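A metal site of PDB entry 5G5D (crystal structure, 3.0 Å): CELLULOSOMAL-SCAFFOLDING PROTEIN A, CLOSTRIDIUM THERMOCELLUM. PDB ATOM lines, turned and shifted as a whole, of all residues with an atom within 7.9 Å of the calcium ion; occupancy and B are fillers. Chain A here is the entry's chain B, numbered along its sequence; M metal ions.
ND2 of Asn 139 sits at hydrogen-bond distance from OE1 of Gln 145, at 2.8 Å. The side-chain carboxylate of Asp 135 is in hydrogen-bond range of the backbone NH of Gly 140. The backbone carbonyl oxygen of Asp 135 is in hydrogen-bond range of the guanidinium group of Arg 138 (2.8 Å). The side-chain carboxylate (OD2) of Asp 135 sits at hydrogen-bond distance from the side-chain hydroxyl (OH) of Tyr 130. The side-chain amide nitrogen of Asn 137 lies close to the side-chain amide nitrogen of Gln 145. The side-chain carboxylate (OD2) of Asp 146 sits close to the backbone NH (N) of Asn 143, 2.8 Å away. The side-chain carboxylate (OD1) of Asp 146 sits close to the backbone NH (N) of Ile 136 (3.5 Å).
Within 4 Å of the calcium ion: Asp 135, Asn 137, Asn 139, Ala 141 and Asp 146. The nearest printed residue that does not touch the calcium ion is Ile 142 (4.2 Å).
The calcium ion is bound by the backbone carbonyl oxygen (O) of Ala 141, the side-chain amide oxygen (OD1) of Asn 139, the side-chain carboxylate (OD1) of Asp 135, the side-chain amide oxygen (OD1) of Asn 137, the side-chain carboxylate (OD1) of Asp 146 and the side-chain carboxylate (OD2) of Asp 146.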
ATOM      1  N   ALA A 123      16.582 -23.246  13.862  1.00  0.00           N
ATOM      2  CA  ALA A 123      16.039 -24.382  14.593  1.00  0.00           C
ATOM      3  C   ALA A 123      15.942 -25.554  13.627  1.00  0.00           C
ATOM      4  O   ALA A 123      15.314 -25.440  12.574  1.00  0.00           O
ATOM      5  CB  ALA A 123      14.665 -24.067  15.178  1.00  0.00           C
ATOM      6  N   TYR A 130      12.087 -25.862  17.652  1.00  0.00           N
ATOM      7  CA  TYR A 130      11.656 -26.308  16.329  1.00  0.00           C
ATOM      8  C   TYR A 130      10.171 -26.647  16.316  1.00  0.00           C
ATOM      9  O   TYR A 130       9.700 -27.425  17.147  1.00  0.00           O
ATOM     10  CB  TYR A 130      12.460 -27.534  15.883  1.00  0.00           C
ATOM     11  CG  TYR A 130      12.045 -28.090  14.530  1.00  0.00           C
ATOM     12  CD1 TYR A 130      12.596 -27.595  13.364  1.00  0.00           C
ATOM     13  CD2 TYR A 130      11.086 -29.094  14.437  1.00  0.00           C
ATOM     14  CE1 TYR A 130      12.207 -28.090  12.122  1.00  0.00           C
ATOM     15  CE2 TYR A 130      10.689 -29.593  13.207  1.00  0.00           C
ATOM     16  CZ  TYR A 130      11.261 -29.092  12.047  1.00  0.00           C
ATOM     17  OH  TYR A 130      10.876 -29.589  10.835  1.00  0.00           O
ATOM     18  N   GLU A 132       7.283 -27.965  13.441  1.00  0.00           N
ATOM     19  CA  GLU A 132       7.244 -28.589  12.110  1.00  0.00           C
ATOM     20  C   GLU A 132       6.502 -27.757  11.058  1.00  0.00           C
ATOM     21  O   GLU A 132       6.917 -27.720   9.899  1.00  0.00           O
ATOM     22  CB  GLU A 132       6.640 -29.999  12.185  1.00  0.00           C
ATOM     23  CG  GLU A 132       6.920 -30.873  10.967  1.00  0.00           C
ATOM     24  CD  GLU A 132       6.198 -32.206  11.027  1.00  0.00           C
ATOM     25  OE1 GLU A 132       6.301 -32.905  12.056  1.00  0.00           O
ATOM     26  OE2 GLU A 132       5.522 -32.558  10.037  1.00  0.00           O
ATOM     27  N   LEU A 134       6.220 -24.456  11.014  1.00  0.00           N
ATOM     28  CA  LEU A 134       7.080 -23.299  10.706  1.00  0.00           C
ATOM     29  C   LEU A 134       8.354 -23.658   9.923  1.00  0.00           C
ATOM     30  O   LEU A 134       9.054 -22.766   9.455  1.00  0.00           O
ATOM     31  CB  LEU A 134       7.440 -22.519  11.980  1.00  0.00           C
ATOM     32  CG  LEU A 134       6.298 -21.741  12.632  1.00  0.00           C
ATOM     33  CD1 LEU A 134       6.762 -21.154  13.958  1.00  0.00           C
ATOM     34  CD2 LEU A 134       5.770 -20.654  11.710  1.00  0.00           C
ATOM     35  N   ASP A 135       8.652 -24.951   9.816  1.00  0.00           N
ATOM     36  CA  ASP A 135       9.566 -25.456   8.793  1.00  0.00           C
ATOM     37  C   ASP A 135       8.720 -25.621   7.518  1.00  0.00           C
ATOM     38  O   ASP A 135       8.166 -26.695   7.278  1.00  0.00           O
ATOM     39  CB  ASP A 135      10.191 -26.783   9.247  1.00  0.00           C
ATOM     40  CG  ASP A 135      11.156 -27.388   8.229  1.00  0.00           C
ATOM     41  OD1 ASP A 135      11.640 -26.671   7.331  1.00  0.00           O
ATOM     42  OD2 ASP A 135      11.435 -28.598   8.354  1.00  0.00           O
ATOM     43  N   ILE A 136       8.632 -24.558   6.720  1.00  0.00           N
ATOM     44  CA  ILE A 136       7.621 -24.474   5.632  1.00  0.00           C
ATOM     45  C   ILE A 136       7.835 -25.578   4.605  1.00  0.00           C
ATOM     46  O   ILE A 136       6.928 -26.347   4.313  1.00  0.00           O
ATOM     47  CB  ILE A 136       7.614 -23.074   4.941  1.00  0.00           C
ATOM     48  CG1 ILE A 136       6.853 -22.015   5.746  1.00  0.00           C
ATOM     49  CG2 ILE A 136       6.907 -23.125   3.588  1.00  0.00           C
ATOM     50  CD1 ILE A 136       7.348 -21.758   7.149  1.00  0.00           C
ATOM     51  N   ASN A 137       9.050 -25.634   4.053  1.00  0.00           N
ATOM     52  CA  ASN A 137       9.430 -26.649   3.063  1.00  0.00           C
ATOM     53  C   ASN A 137       9.600 -28.072   3.632  1.00  0.00           C
ATOM     54  O   ASN A 137       9.660 -29.038   2.864  1.00  0.00           O
ATOM     55  CB  ASN A 137      10.716 -26.237   2.322  1.00  0.00           C
ATOM     56  CG  ASN A 137      11.877 -25.949   3.274  1.00  0.00           C
ATOM     57  OD1 ASN A 137      11.938 -26.481   4.381  1.00  0.00           O
ATOM     58  ND2 ASN A 137      12.777 -25.076   2.861  1.00  0.00           N
ATOM     59  N   ARG A 138       9.715 -28.181   4.958  1.00  0.00           N
ATOM     60  CA  ARG A 138       9.862 -29.458   5.672  1.00  0.00           C
ATOM     61  C   ARG A 138      11.225 -30.132   5.454  1.00  0.00           C
ATOM     62  O   ARG A 138      11.358 -31.344   5.676  1.00  0.00           O
ATOM     63  CB  ARG A 138       8.719 -30.439   5.358  1.00  0.00           C
ATOM     64  CG  ARG A 138       7.339 -29.954   5.760  1.00  0.00           C
ATOM     65  CD  ARG A 138       7.150 -30.015   7.275  1.00  0.00           C
ATOM     66  NE  ARG A 138       5.734 -29.935   7.630  1.00  0.00           N
ATOM     67  CZ  ARG A 138       4.990 -28.832   7.600  1.00  0.00           C
ATOM     68  NH1 ARG A 138       5.488 -27.660   7.225  1.00  0.00           N
ATOM     69  NH2 ARG A 138       3.709 -28.905   7.953  1.00  0.00           N
ATOM     70  N   ASN A 139      12.244 -29.367   5.055  1.00  0.00           N
ATOM     71  CA  ASN A 139      13.565 -29.939   4.750  1.00  0.00           C
ATOM     72  C   ASN A 139      14.477 -30.130   5.982  1.00  0.00           C
ATOM     73  O   ASN A 139      15.637 -30.533   5.826  1.00  0.00           O
ATOM     74  CB  ASN A 139      14.278 -29.144   3.633  1.00  0.00           C
ATOM     75  CG  ASN A 139      14.825 -27.798   4.083  1.00  0.00           C
ATOM     76  OD1 ASN A 139      14.575 -27.351   5.200  1.00  0.00           O
ATOM     77  ND2 ASN A 139      15.562 -27.141   3.199  1.00  0.00           N
ATOM     78  N   GLY A 140      13.961 -29.833   7.178  1.00  0.00           N
ATOM     79  CA  GLY A 140      14.628 -30.192   8.433  1.00  0.00           C
ATOM     80  C   GLY A 140      15.092 -29.034   9.293  1.00  0.00           C
ATOM     81  O   GLY A 140      15.338 -29.228  10.480  1.00  0.00           O
ATOM     82  N   ALA A 141      15.219 -27.854   8.709  1.00  0.00           N
ATOM     83  CA  ALA A 141      15.726 -26.671   9.410  1.00  0.00           C
ATOM     84  C   ALA A 141      14.888 -25.439   9.090  1.00  0.00           C
ATOM     85  O   ALA A 141      14.513 -25.232   7.937  1.00  0.00           O
ATOM     86  CB  ALA A 141      17.179 -26.435   9.027  1.00  0.00           C
ATOM     87  N   ILE A 142      14.592 -24.631  10.104  1.00  0.00           N
ATOM     88  CA  ILE A 142      13.879 -23.359   9.926  1.00  0.00           C
ATOM     89  C   ILE A 142      14.904 -22.267   9.678  1.00  0.00           C
ATOM     90  O   ILE A 142      15.670 -21.926  10.590  1.00  0.00           O
ATOM     91  CB  ILE A 142      12.997 -23.028  11.148  1.00  0.00           C
ATOM     92  CG1 ILE A 142      11.875 -24.055  11.275  1.00  0.00           C
ATOM     93  CG2 ILE A 142      12.427 -21.616  11.045  1.00  0.00           C
ATOM     94  CD1 ILE A 142      11.477 -24.365  12.700  1.00  0.00           C
ATOM     95  N   ASN A 143      14.927 -21.714   8.465  1.00  0.00           N
ATOM     96  CA  ASN A 143      15.969 -20.765   8.042  1.00  0.00           C
ATOM     97  C   ASN A 143      15.469 -19.778   6.977  1.00  0.00           C
ATOM     98  O   ASN A 143      14.262 -19.689   6.747  1.00  0.00           O
ATOM     99  CB  ASN A 143      17.223 -21.558   7.593  1.00  0.00           C
ATOM    100  CG  ASN A 143      16.938 -22.532   6.458  1.00  0.00           C
ATOM    101  OD1 ASN A 143      16.122 -22.284   5.578  1.00  0.00           O
ATOM    102  ND2 ASN A 143      17.653 -23.654   6.471  1.00  0.00           N
ATOM    103  N   MET A 144      16.379 -19.055   6.330  1.00  0.00           N
ATOM    104  CA  MET A 144      16.036 -18.068   5.299  1.00  0.00           C
ATOM    105  C   MET A 144      15.220 -18.633   4.138  1.00  0.00           C
ATOM    106  O   MET A 144      14.400 -17.918   3.550  1.00  0.00           O
ATOM    107  CB  MET A 144      17.293 -17.390   4.751  1.00  0.00           C
ATOM    108  CG  MET A 144      17.048 -16.109   3.973  1.00  0.00           C
ATOM    109  SD  MET A 144      16.229 -14.834   4.944  1.00  0.00           S
ATOM    110  CE  MET A 144      17.502 -14.506   6.163  1.00  0.00           C
ATOM    111  N   GLN A 145      15.453 -19.901   3.810  1.00  0.00           N
ATOM    112  CA  GLN A 145      14.710 -20.589   2.741  1.00  0.00           C
ATOM    113  C   GLN A 145      13.195 -20.537   2.949  1.00  0.00           C
ATOM    114  O   GLN A 145      12.446 -20.375   2.002  1.00  0.00           O
ATOM    115  CB  GLN A 145      15.168 -22.048   2.627  1.00  0.00           C
ATOM    116  CG  GLN A 145      14.833 -22.716   1.305  1.00  0.00           C
ATOM    117  CD  GLN A 145      15.245 -24.168   1.260  1.00  0.00           C
ATOM    118  OE1 GLN A 145      16.109 -24.619   2.018  1.00  0.00           O
ATOM    119  NE2 GLN A 145      14.601 -24.928   0.373  1.00  0.00           N
ATOM    120  N   ASP A 146      12.778 -20.663   4.215  1.00  0.00           N
ATOM    121  CA  ASP A 146      11.357 -20.681   4.575  1.00  0.00           C
ATOM    122  C   ASP A 146      10.786 -19.273   4.676  1.00  0.00           C
ATOM    123  O   ASP A 146       9.622 -19.058   4.333  1.00  0.00           O
ATOM    124  CB  ASP A 146      11.153 -21.391   5.912  1.00  0.00           C
ATOM    125  CG  ASP A 146      11.924 -22.676   6.018  1.00  0.00           C
ATOM    126  OD1 ASP A 146      11.624 -23.628   5.273  1.00  0.00           O
ATOM    127  OD2 ASP A 146      12.867 -22.720   6.836  1.00  0.00           O
ATOM    128  N   ILE A 147      11.597 -18.341   5.177  1.00  0.00           N
ATOM    129  CA  ILE A 147      11.214 -16.931   5.306  1.00  0.00           C
ATOM    130  C   ILE A 147      10.885 -16.347   3.923  1.00  0.00           C
ATOM    131  O   ILE A 147       9.884 -15.634   3.774  1.00  0.00           O
ATOM    132  CB  ILE A 147      12.320 -16.097   6.004  1.00  0.00           C
ATOM    133  CG1 ILE A 147      12.452 -16.528   7.471  1.00  0.00           C
ATOM    134  CG2 ILE A 147      12.031 -14.595   5.918  1.00  0.00           C
ATOM    135  CD1 ILE A 147      13.741 -16.095   8.144  1.00  0.00           C
ATOM    136  N   ILE A 149       9.758 -17.986   1.412  1.00  0.00           N
ATOM    137  CA  ILE A 149       8.480 -18.575   0.992  1.00  0.00           C
ATOM    138  C   ILE A 149       7.321 -17.737   1.539  1.00  0.00           C
ATOM    139  O   ILE A 149       6.294 -17.582   0.874  1.00  0.00           O
ATOM    140  CB  ILE A 149       8.316 -20.051   1.434  1.00  0.00           C
ATOM    141  CG1 ILE A 149       9.472 -20.925   0.916  1.00  0.00           C
ATOM    142  CG2 ILE A 149       7.008 -20.628   0.918  1.00  0.00           C
ATOM    143  CD1 ILE A 149       9.580 -22.295   1.570  1.00  0.00           C
HETATM  144 CA    CA M   1      13.401 -25.466   6.166  1.00  0.00          CA
